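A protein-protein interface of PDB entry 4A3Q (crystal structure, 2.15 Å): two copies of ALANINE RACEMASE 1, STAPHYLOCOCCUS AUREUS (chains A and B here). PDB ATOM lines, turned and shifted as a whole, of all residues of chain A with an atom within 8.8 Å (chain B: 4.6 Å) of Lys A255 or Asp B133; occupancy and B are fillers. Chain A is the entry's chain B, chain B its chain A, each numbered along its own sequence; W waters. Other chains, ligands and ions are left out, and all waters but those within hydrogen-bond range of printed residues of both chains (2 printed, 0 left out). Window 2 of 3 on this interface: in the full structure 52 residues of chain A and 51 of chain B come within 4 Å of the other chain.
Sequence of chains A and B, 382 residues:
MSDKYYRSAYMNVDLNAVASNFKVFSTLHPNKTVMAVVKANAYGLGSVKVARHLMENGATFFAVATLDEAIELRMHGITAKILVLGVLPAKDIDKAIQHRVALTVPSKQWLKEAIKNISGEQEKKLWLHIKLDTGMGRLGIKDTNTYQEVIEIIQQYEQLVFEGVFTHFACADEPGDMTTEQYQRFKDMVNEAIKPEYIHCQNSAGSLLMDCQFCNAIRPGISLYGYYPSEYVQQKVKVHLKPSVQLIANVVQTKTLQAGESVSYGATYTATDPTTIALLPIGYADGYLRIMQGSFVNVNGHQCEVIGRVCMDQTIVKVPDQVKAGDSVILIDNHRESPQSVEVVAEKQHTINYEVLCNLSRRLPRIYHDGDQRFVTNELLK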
ATOM      1  N   VAL A 251       2.344   2.153  -2.606  1.00  0.00           N
ATOM      2  CA  VAL A 251       3.802   2.298  -2.657  1.00  0.00           C
ATOM      3  C   VAL A 251       4.357   1.617  -3.912  1.00  0.00           C
ATOM      4  O   VAL A 251       4.028   0.475  -4.174  1.00  0.00           O
ATOM      5  CB  VAL A 251       4.449   1.695  -1.381  1.00  0.00           C
ATOM      6  CG1 VAL A 251       5.973   1.812  -1.449  1.00  0.00           C
ATOM      7  CG2 VAL A 251       3.937   2.425  -0.141  1.00  0.00           C
ATOM      8  N   VAL A 252       5.163   2.300  -4.724  1.00  0.00           N
ATOM      9  CA  VAL A 252       5.759   1.551  -5.853  1.00  0.00           C
ATOM     10  C   VAL A 252       7.214   1.160  -5.604  1.00  0.00           C
ATOM     11  O   VAL A 252       7.744   0.293  -6.277  1.00  0.00           O
ATOM     12  CB  VAL A 252       5.622   2.254  -7.249  1.00  0.00           C
ATOM     13  CG1 VAL A 252       4.128   2.253  -7.732  1.00  0.00           C
ATOM     14  CG2 VAL A 252       6.217   3.656  -7.212  1.00  0.00           C
ATOM     15  N   GLN A 253       7.850   1.816  -4.648  1.00  0.00           N
ATOM     16  CA  GLN A 253       9.249   1.536  -4.301  1.00  0.00           C
ATOM     17  C   GLN A 253       9.537   2.137  -2.944  1.00  0.00           C
ATOM     18  O   GLN A 253       9.063   3.235  -2.614  1.00  0.00           O
ATOM     19  CB  GLN A 253      10.252   2.080  -5.366  1.00  0.00           C
ATOM     20  CG  GLN A 253      11.767   1.804  -5.045  1.00  0.00           C
ATOM     21  CD  GLN A 253      12.764   2.295  -6.111  1.00  0.00           C
ATOM     22  OE1 GLN A 253      12.480   3.201  -6.890  1.00  0.00           O
ATOM     23  NE2 GLN A 253      13.935   1.689  -6.136  1.00  0.00           N
ATOM     24  N   THR A 254      10.293   1.397  -2.142  1.00  0.00           N
ATOM     25  CA  THR A 254      10.823   1.924  -0.888  1.00  0.00           C
ATOM     26  C   THR A 254      12.342   2.037  -0.981  1.00  0.00           C
ATOM     27  O   THR A 254      13.001   1.219  -1.605  1.00  0.00           O
ATOM     28  CB  THR A 254      10.456   1.049   0.319  1.00  0.00           C
ATOM     29  OG1 THR A 254      11.014  -0.260   0.151  1.00  0.00           O
ATOM     30  CG2 THR A 254       8.941   0.928   0.437  1.00  0.00           C
ATOM     31  N   LYS A 255      12.885   3.062  -0.352  1.00  0.00           N
ATOM     32  CA  LYS A 255      14.299   3.310  -0.433  1.00  0.00           C
ATOM     33  C   LYS A 255      14.746   3.663   0.953  1.00  0.00           C
ATOM     34  O   LYS A 255      14.004   4.299   1.696  1.00  0.00           O
ATOM     35  CB  LYS A 255      14.568   4.470  -1.396  1.00  0.00           C
ATOM     36  CG  LYS A 255      16.013   4.599  -1.812  1.00  0.00           C
ATOM     37  CD  LYS A 255      16.131   5.290  -3.174  1.00  0.00           C
ATOM     38  CE  LYS A 255      16.009   4.292  -4.311  1.00  0.00           C
ATOM     39  NZ  LYS A 255      16.202   4.984  -5.595  1.00  0.00           N
ATOM     40  N   THR A 256      15.942   3.224   1.319  1.00  0.00           N
ATOM     41  CA  THR A 256      16.565   3.681   2.562  1.00  0.00           C
ATOM     42  C   THR A 256      17.638   4.722   2.226  1.00  0.00           C
ATOM     43  O   THR A 256      18.457   4.510   1.324  1.00  0.00           O
ATOM     44  CB  THR A 256      17.170   2.509   3.341  1.00  0.00           C
ATOM     45  OG1 THR A 256      17.955   1.719   2.442  1.00  0.00           O
ATOM     46  CG2 THR A 256      16.073   1.610   3.928  1.00  0.00           C
ATOM     47  N   LEU A 257      17.467   5.840   2.800  1.00  0.00           N
ATOM     48  CA  LEU A 257      18.442   6.849   2.560  1.00  0.00           C
ATOM     49  C   LEU A 257      18.972   7.390   3.866  1.00  0.00           C
ATOM     50  O   LEU A 257      19.214   6.648   4.796  1.00  0.00           O
ATOM     51  CB  LEU A 257      17.917   7.963   1.680  1.00  0.00           C
ATOM     52  N   PRO A 274      18.688   7.897   9.080  1.00  0.00           N
ATOM     53  CA  PRO A 274      18.472   6.448   9.179  1.00  0.00           C
ATOM     54  C   PRO A 274      17.084   5.970   8.669  1.00  0.00           C
ATOM     55  O   PRO A 274      16.615   4.895   9.085  1.00  0.00           O
ATOM     56  CB  PRO A 274      18.624   6.173  10.692  1.00  0.00           C
ATOM     57  CG  PRO A 274      18.942   7.548  11.354  1.00  0.00           C
ATOM     58  CD  PRO A 274      19.439   8.417  10.234  1.00  0.00           C
ATOM     59  N   THR A 275      16.471   6.719   7.743  1.00  0.00           N
ATOM     60  CA  THR A 275      15.035   6.575   7.437  1.00  0.00           C
ATOM     61  C   THR A 275      14.659   6.011   6.055  1.00  0.00           C
ATOM     62  O   THR A 275      15.254   6.369   5.032  1.00  0.00           O
ATOM     63  CB  THR A 275      14.277   7.928   7.618  1.00  0.00           C
ATOM     64  OG1 THR A 275      14.279   8.654   6.381  1.00  0.00           O
ATOM     65  CG2 THR A 275      14.922   8.795   8.725  1.00  0.00           C
ATOM     66  N   THR A 276      13.646   5.142   6.055  1.00  0.00           N
ATOM     67  CA  THR A 276      13.024   4.631   4.848  1.00  0.00           C
ATOM     68  C   THR A 276      12.070   5.675   4.247  1.00  0.00           C
ATOM     69  O   THR A 276      11.406   6.410   4.961  1.00  0.00           O
ATOM     70  CB  THR A 276      12.233   3.335   5.138  1.00  0.00           C
ATOM     71  OG1 THR A 276      13.061   2.418   5.853  1.00  0.00           O
ATOM     72  CG2 THR A 276      11.779   2.658   3.848  1.00  0.00           C
ATOM     73  N   ILE A 277      12.032   5.738   2.925  1.00  0.00           N
ATOM     74  CA  ILE A 277      11.053   6.539   2.211  1.00  0.00           C
ATOM     75  C   ILE A 277      10.297   5.659   1.241  1.00  0.00           C
ATOM     76  O   ILE A 277      10.808   4.619   0.811  1.00  0.00           O
ATOM     77  CB  ILE A 277      11.704   7.712   1.443  1.00  0.00           C
ATOM     78  CG1 ILE A 277      12.704   7.202   0.401  1.00  0.00           C
ATOM     79  CG2 ILE A 277      12.369   8.671   2.418  1.00  0.00           C
ATOM     80  CD1 ILE A 277      13.214   8.304  -0.503  1.00  0.00           C
ATOM     81  N   ALA A 278       9.073   6.084   0.922  1.00  0.00           N
ATOM     82  CA  ALA A 278       8.177   5.358   0.006  1.00  0.00           C
ATOM     83  C   ALA A 278       7.752   6.287  -1.142  1.00  0.00           C
ATOM     84  O   ALA A 278       7.429   7.461  -0.940  1.00  0.00           O
ATOM     85  CB  ALA A 278       6.960   4.852   0.744  1.00  0.00           C
ATOM     86  N   LEU A 279       7.766   5.747  -2.347  1.00  0.00           N
ATOM     87  CA  LEU A 279       7.416   6.520  -3.516  1.00  0.00           C
ATOM     88  C   LEU A 279       6.015   6.130  -3.951  1.00  0.00           C
ATOM     89  O   LEU A 279       5.714   4.952  -4.074  1.00  0.00           O
ATOM     90  CB  LEU A 279       8.416   6.255  -4.643  1.00  0.00           C
ATOM     91  CG  LEU A 279       9.613   7.220  -4.670  1.00  0.00           C
ATOM     92  CD1 LEU A 279      10.571   7.042  -3.509  1.00  0.00           C
ATOM     93  CD2 LEU A 279      10.351   7.034  -5.958  1.00  0.00           C
ATOM     94  N   ILE A 307       7.349  14.200   2.347  1.00  0.00           N
ATOM     95  CA  ILE A 307       8.627  14.933   2.374  1.00  0.00           C
ATOM     96  C   ILE A 307       9.113  15.332   0.985  1.00  0.00           C
ATOM     97  O   ILE A 307       8.736  14.723  -0.011  1.00  0.00           O
ATOM     98  CB  ILE A 307       9.717  14.141   3.125  1.00  0.00           C
ATOM     99  CG1 ILE A 307       9.881  12.734   2.529  1.00  0.00           C
ATOM    100  CG2 ILE A 307       9.388  14.070   4.651  1.00  0.00           C
ATOM    101  CD1 ILE A 307      11.167  12.008   3.015  1.00  0.00           C
ATOM    102  N   ILE A 316       6.572  11.680  -2.291  1.00  0.00           N
ATOM    103  CA  ILE A 316       7.463  10.914  -1.425  1.00  0.00           C
ATOM    104  C   ILE A 316       7.032  10.985   0.035  1.00  0.00           C
ATOM    105  O   ILE A 316       6.716  12.038   0.551  1.00  0.00           O
ATOM    106  CB  ILE A 316       8.965  11.265  -1.635  1.00  0.00           C
ATOM    107  CG1 ILE A 316       9.388  10.834  -3.056  1.00  0.00           C
ATOM    108  CG2 ILE A 316       9.840  10.524  -0.623  1.00  0.00           C
ATOM    109  CD1 ILE A 316      10.673  11.542  -3.594  1.00  0.00           C
ATOM    110  N   VAL A 317       7.024   9.827   0.676  1.00  0.00           N
ATOM    111  CA  VAL A 317       6.556   9.715   2.040  1.00  0.00           C
ATOM    112  C   VAL A 317       7.645   9.111   2.947  1.00  0.00           C
ATOM    113  O   VAL A 317       8.260   8.124   2.582  1.00  0.00           O
ATOM    114  CB  VAL A 317       5.270   8.839   2.056  1.00  0.00           C
ATOM    115  CG1 VAL A 317       4.769   8.661   3.468  1.00  0.00           C
ATOM    116  CG2 VAL A 317       4.184   9.510   1.203  1.00  0.00           C
ATOM    117  N   LYS A 318       7.885   9.713   4.115  1.00  0.00           N
ATOM    118  CA  LYS A 318       8.783   9.122   5.130  1.00  0.00           C
ATOM    119  C   LYS A 318       8.046   7.994   5.864  1.00  0.00           C
ATOM    120  O   LYS A 318       7.052   8.258   6.528  1.00  0.00           O
ATOM    121  CB  LYS A 318       9.232  10.187   6.141  1.00  0.00           C
ATOM    122  CG  LYS A 318      10.232   9.674   7.212  1.00  0.00           C
ATOM    123  CD  LYS A 318      10.598  10.757   8.252  1.00  0.00           C
ATOM    124  CE  LYS A 318      11.525  10.206   9.372  1.00  0.00           C
ATOM    125  NZ  LYS A 318      10.851   9.626  10.606  1.00  0.00           N
ATOM    126  N   VAL A 319       8.521   6.751   5.734  1.00  0.00           N
ATOM    127  CA  VAL A 319       7.803   5.587   6.267  1.00  0.00           C
ATOM    128  C   VAL A 319       8.601   4.780   7.310  1.00  0.00           C
ATOM    129  O   VAL A 319       9.828   4.912   7.384  1.00  0.00           O
ATOM    130  CB  VAL A 319       7.310   4.631   5.129  1.00  0.00           C
ATOM    131  CG1 VAL A 319       6.204   5.303   4.292  1.00  0.00           C
ATOM    132  CG2 VAL A 319       8.462   4.142   4.224  1.00  0.00           C
ATOM    133  N   PRO A 320       7.894   3.972   8.143  1.00  0.00           N
ATOM    134  CA  PRO A 320       8.561   2.953   8.969  1.00  0.00           C
ATOM    135  C   PRO A 320       9.220   1.889   8.084  1.00  0.00           C
ATOM    136  O   PRO A 320       8.803   1.693   6.944  1.00  0.00           O
ATOM    137  CB  PRO A 320       7.414   2.323   9.771  1.00  0.00           C
ATOM    138  CG  PRO A 320       6.310   3.293   9.742  1.00  0.00           C
ATOM    139  CD  PRO A 320       6.479   4.155   8.516  1.00  0.00           C
ATOM    140  N   ASP A 321      10.216   1.189   8.625  1.00  0.00           N
ATOM    141  CA  ASP A 321      11.078   0.301   7.849  1.00  0.00           C
ATOM    142  C   ASP A 321      10.377  -0.929   7.284  1.00  0.00           C
ATOM    143  O   ASP A 321      10.847  -1.515   6.302  1.00  0.00           O
ATOM    144  CB  ASP A 321      12.320  -0.102   8.678  1.00  0.00           C
ATOM    145  CG  ASP A 321      13.127   1.117   9.165  1.00  0.00           C
ATOM    146  OD1 ASP A 321      13.254   2.113   8.413  1.00  0.00           O
ATOM    147  OD2 ASP A 321      13.641   1.082  10.310  1.00  0.00           O
ATOM    148  N   VAL A 323       7.372  -0.897   5.869  1.00  0.00           N
ATOM    149  CA  VAL A 323       6.553  -0.555   4.702  1.00  0.00           C
ATOM    150  C   VAL A 323       7.278  -1.038   3.447  1.00  0.00           C
ATOM    151  O   VAL A 323       8.484  -0.799   3.304  1.00  0.00           O
ATOM    152  CB  VAL A 323       6.277   0.967   4.639  1.00  0.00           C
ATOM    153  CG1 VAL A 323       5.701   1.399   3.253  1.00  0.00           C
ATOM    154  CG2 VAL A 323       5.363   1.392   5.801  1.00  0.00           C
ATOM    155  N   LYS A 324       6.550  -1.744   2.572  1.00  0.00           N
ATOM    156  CA  LYS A 324       7.085  -2.196   1.279  1.00  0.00           C
ATOM    157  C   LYS A 324       6.205  -1.856   0.056  1.00  0.00           C
ATOM    158  O   LYS A 324       5.027  -1.496   0.196  1.00  0.00           O
ATOM    159  CB  LYS A 324       7.397  -3.704   1.295  1.00  0.00           C
ATOM    160  CG  LYS A 324       6.440  -4.536   2.123  1.00  0.00           C
ATOM    161  CD  LYS A 324       6.742  -6.037   2.031  1.00  0.00           C
ATOM    162  CE  LYS A 324       5.466  -6.861   2.248  1.00  0.00           C
ATOM    163  NZ  LYS A 324       4.412  -6.560   1.230  1.00  0.00           N
ATOM    164  N   ALA A 325       6.790  -2.002  -1.132  1.00  0.00           N
ATOM    165  CA  ALA A 325       6.067  -1.845  -2.396  1.00  0.00           C
ATOM    166  C   ALA A 325       4.808  -2.666  -2.374  1.00  0.00           C
ATOM    167  O   ALA A 325       4.842  -3.825  -1.953  1.00  0.00           O
ATOM    168  CB  ALA A 325       6.940  -2.273  -3.565  1.00  0.00           C
ATOM    169  N   LYS B 131      15.754   2.703 -14.946  1.00  0.00           N
ATOM    170  CA  LYS B 131      15.864   4.005 -14.298  1.00  0.00           C
ATOM    171  C   LYS B 131      16.935   3.945 -13.239  1.00  0.00           C
ATOM    172  O   LYS B 131      16.908   3.095 -12.382  1.00  0.00           O
ATOM    173  CB  LYS B 131      14.542   4.398 -13.652  1.00  0.00           C
ATOM    174  CG  LYS B 131      14.594   5.620 -12.721  1.00  0.00           C
ATOM    175  CD  LYS B 131      14.495   6.903 -13.470  1.00  0.00           C
ATOM    176  CE  LYS B 131      14.018   8.059 -12.572  1.00  0.00           C
ATOM    177  NZ  LYS B 131      15.181   8.619 -11.777  1.00  0.00           N
ATOM    178  N   LEU B 132      17.886   4.858 -13.300  1.00  0.00           N
ATOM    179  CA  LEU B 132      18.950   4.904 -12.304  1.00  0.00           C
ATOM    180  C   LEU B 132      18.700   6.076 -11.388  1.00  0.00           C
ATOM    181  O   LEU B 132      18.339   7.160 -11.827  1.00  0.00           O
ATOM    182  CB  LEU B 132      20.326   5.043 -12.977  1.00  0.00           C
ATOM    183  CG  LEU B 132      20.788   3.844 -13.819  1.00  0.00           C
ATOM    184  CD1 LEU B 132      22.185   4.047 -14.394  1.00  0.00           C
ATOM    185  CD2 LEU B 132      20.770   2.580 -12.991  1.00  0.00           C
ATOM    186  N   ASP B 133      18.891   5.833 -10.104  1.00  0.00           N
ATOM    187  CA  ASP B 133      18.911   6.869  -9.090  1.00  0.00           C
ATOM    188  C   ASP B 133      20.371   7.316  -8.941  1.00  0.00           C
ATOM    189  O   ASP B 133      21.176   6.586  -8.368  1.00  0.00           O
ATOM    190  CB  ASP B 133      18.370   6.271  -7.786  1.00  0.00           C
ATOM    191  CG  ASP B 133      18.530   7.190  -6.575  1.00  0.00           C
ATOM    192  OD1 ASP B 133      18.968   8.357  -6.705  1.00  0.00           O
ATOM    193  OD2 ASP B 133      18.196   6.731  -5.464  1.00  0.00           O
ATOM    194  N   THR B 134      20.683   8.514  -9.458  1.00  0.00           N
ATOM    195  CA  THR B 134      22.032   9.084  -9.480  1.00  0.00           C
ATOM    196  C   THR B 134      22.266  10.203  -8.440  1.00  0.00           C
ATOM    197  O   THR B 134      23.151  11.056  -8.608  1.00  0.00           O
ATOM    198  CB  THR B 134      22.410   9.628 -10.896  1.00  0.00           C
ATOM    199  OG1 THR B 134      21.414  10.564 -11.327  1.00  0.00           O
ATOM    200  CG2 THR B 134      22.529   8.486 -11.911  1.00  0.00           C
ATOM    201  N   GLY B 135      21.496  10.190  -7.357  1.00  0.00           N
ATOM    202  CA  GLY B 135      21.731  11.138  -6.280  1.00  0.00           C
ATOM    203  C   GLY B 135      20.503  11.823  -5.726  1.00  0.00           C
ATOM    204  O   GLY B 135      20.580  12.487  -4.688  1.00  0.00           O
ATOM    205  N   MET B 136      19.368  11.678  -6.401  1.00  0.00           N
ATOM    206  CA  MET B 136      18.142  12.346  -5.963  1.00  0.00           C
ATOM    207  C   MET B 136      17.470  11.586  -4.820  1.00  0.00           C
ATOM    208  O   MET B 136      16.615  12.125  -4.127  1.00  0.00           O
ATOM    209  CB  MET B 136      17.166  12.502  -7.139  1.00  0.00           C
ATOM    210  CG  MET B 136      17.613  13.501  -8.201  1.00  0.00           C
ATOM    211  SD  MET B 136      17.888  15.152  -7.502  1.00  0.00           S
ATOM    212  CE  MET B 136      16.197  15.593  -7.055  1.00  0.00           C
ATOM    213  N   GLY B 137      17.849  10.322  -4.648  1.00  0.00           N
ATOM    214  CA  GLY B 137      17.197   9.451  -3.666  1.00  0.00           C
ATOM    215  C   GLY B 137      15.722   9.209  -3.978  1.00  0.00           C
ATOM    216  O   GLY B 137      14.930   9.007  -3.063  1.00  0.00           O
ATOM    217  N   ARG B 138      15.342   9.239  -5.258  1.00  0.00           N
ATOM    218  CA  ARG B 138      13.957   8.969  -5.627  1.00  0.00           C
ATOM    219  C   ARG B 138      13.854   7.641  -6.373  1.00  0.00           C
ATOM    220  O   ARG B 138      14.359   6.624  -5.894  1.00  0.00           O
ATOM    221  CB  ARG B 138      13.363  10.124  -6.440  1.00  0.00           C
ATOM    222  N   LEU B 139      13.202   7.637  -7.531  1.00  0.00           N
ATOM    223  CA  LEU B 139      12.869   6.393  -8.188  1.00  0.00           C
ATOM    224  C   LEU B 139      14.104   5.786  -8.830  1.00  0.00           C
ATOM    225  O   LEU B 139      14.910   6.501  -9.428  1.00  0.00           O
ATOM    226  CB  LEU B 139      11.791   6.624  -9.240  1.00  0.00           C
ATOM    227  CG  LEU B 139      11.051   5.390  -9.759  1.00  0.00           C
ATOM    228  CD1 LEU B 139      10.179   4.721  -8.653  1.00  0.00           C
ATOM    229  CD2 LEU B 139      10.220   5.753 -11.010  1.00  0.00           C
ATOM    230  N   GLY B 140      14.249   4.471  -8.723  1.00  0.00           N
ATOM    231  CA  GLY B 140      15.260   3.785  -9.522  1.00  0.00           C
ATOM    232  C   GLY B 140      16.398   3.142  -8.752  1.00  0.00           C
ATOM    233  O   GLY B 140      16.401   3.121  -7.520  1.00  0.00           O
ATOM    234  N   ILE B 141      17.352   2.605  -9.504  1.00  0.00           N
ATOM    235  CA  ILE B 141      18.412   1.740  -8.955  1.00  0.00           C
ATOM    236  C   ILE B 141      19.621   2.596  -8.627  1.00  0.00           C
ATOM    237  O   ILE B 141      20.128   3.332  -9.497  1.00  0.00           O
ATOM    238  CB  ILE B 141      18.812   0.656  -9.961  1.00  0.00           C
ATOM    239  CG1 ILE B 141      17.611  -0.266 -10.201  1.00  0.00           C
ATOM    240  CG2 ILE B 141      20.102  -0.096  -9.482  1.00  0.00           C
ATOM    241  CD1 ILE B 141      17.781  -1.269 -11.320  1.00  0.00           C
ATOM    242  N   LYS B 142      20.064   2.561  -7.370  1.00  0.00           N
ATOM    243  CA  LYS B 142      21.172   3.470  -7.002  1.00  0.00           C
ATOM    244  C   LYS B 142      22.538   2.788  -6.970  1.00  0.00           C
ATOM    245  O   LYS B 142      23.575   3.463  -6.972  1.00  0.00           O
ATOM    246  CB  LYS B 142      20.882   4.237  -5.706  1.00  0.00           C
ATOM    247  CG  LYS B 142      20.657   3.381  -4.493  1.00  0.00           C
ATOM    248  CD  LYS B 142      20.475   4.262  -3.230  1.00  0.00           C
ATOM    249  CE  LYS B 142      21.180   3.641  -2.018  1.00  0.00           C
ATOM    250  NZ  LYS B 142      20.575   2.340  -1.568  1.00  0.00           N
ATOM    251  N   MET B 189      27.969   4.868 -13.750  1.00  0.00           N
ATOM    252  CA  MET B 189      27.155   3.657 -13.616  1.00  0.00           C
ATOM    253  C   MET B 189      26.950   3.019 -15.000  1.00  0.00           C
ATOM    254  O   MET B 189      27.172   1.844 -15.165  1.00  0.00           O
ATOM    255  CB  MET B 189      25.806   3.954 -12.943  1.00  0.00           C
ATOM    256  CG  MET B 189      25.898   4.413 -11.481  1.00  0.00           C
ATOM    257  SD  MET B 189      24.235   4.739 -10.831  1.00  0.00           S
ATOM    258  CE  MET B 189      23.762   3.036 -10.492  1.00  0.00           C
HETATM  259  O   HOH W   1      17.883   1.193  -0.552  1.00  0.00           O
HETATM  260  O   HOH W   2      16.068   0.083  -6.837  1.00  0.00           O
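NZ of Lys B131 lies within hydrogen-bond range of O of Leu B139 (3.2 Å). The side-chain carboxylate (OD1) of Asp B133 is in hydrogen-bond range of the backbone NH (N) of Met B136. N of Asp B133 is in hydrogen-bond range of O of Ile B141 (2.9 Å). The backbone carbonyl oxygen (O) of Leu A279 lies within hydrogen-bond range of the backbone NH (N) of Val A252, 2.8 Å away. O of Gln A253 sits at hydrogen-bond distance from N of Leu A279 (2.8 Å). The backbone NH of Ile A277 is in hydrogen-bond range of the backbone carbonyl oxygen of Lys A255 (2.7 Å).
NZ of Lys A255 lies within salt-bridge range of OD2 of Asp B133 (2.7 Å). The backbone carbonyl oxygen (O) of Arg B138 is in hydrogen-bond range of the side-chain amino group (NZ) of Lys A255 (2.5 Å). OE1 of Gln A253 lies within hydrogen-bond range of N of Gly B140, at 2.8 Å. The side-chain amino group (NZ) of Lys A255 lies within hydrogen-bond range of the backbone carbonyl oxygen (O) of Gly B140 (2.7 Å).
Among the printed residues, pairs that only touch across the chains: Ile A277 with Gly B137 (3.2 Å), Gln A253 with Leu B139 (3.3 Å), Leu A279 with Leu B139 (3.3 Å), Leu A279 with Arg B138 (3.6 Å), Lys A255 with Gly B137 (3.9 Å) and Lys A255 with Leu B139 (3.9 Å).
No position is printed for both chains.
Of the 13 printed residues of chain B, 5 touch a printed residue of chain A. Hydrophobic or aromatic side chains of chain B that line the printed part of chain A: Leu B139. Hydrophobic or aromatic side chains of chain A that line the printed part of chain B: Ile A277 and Leu A279. Among the printed residues, Asp or Glu carboxylates within 4 Å of a Lys or Arg side-chain nitrogen of the other chain: Lys A255 with Asp B133 (2.7 Å).
Water W2 bridges the side-chain amide nitrogen of Gln A253 (2.8 Å) and the backbone carbonyl oxygen of Gly B140 (3.1 Å). Water W1 lies within hydrogen-bond range of OG1 of Thr A256 (3.0 Å) and NZ of Lys B142 (3.1 Å).
Of chain B, only Asp B133, Gly B137, Arg B138, Leu B139 and Gly B140 come within 4 Å of Lys A255. Asp B133 touches just one residue of chain A: Lys A255. Gly B137 touches just these residues of chain A: Lys A255 (3.9 Å) and Ile A277 (3.2 Å). Of chain A, only Gln A253 and Lys A255 come within 4 Å of Gly B140. Of the printed residues of chain B, Gln A253 touches Leu B139 (3.3 Å) and Gly B140 (2.8 Å). Of the printed residues of chain B, Leu A279 touches Arg B138 and Leu B139. Of the printed residues of chain B, Ile A277 touches Gly B137 (3.2 Å). Of the printed residues of chain A, Arg B138 touches Lys A255 (2.5 Å) and Leu A279 (3.6 Å). The nearest residue of chain B that does not touch Lys A255 is Lys B142 (4.5 Å). The nearest residue of chain A that does not touch Asp B133 is Gln A253 (6.6 Å).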
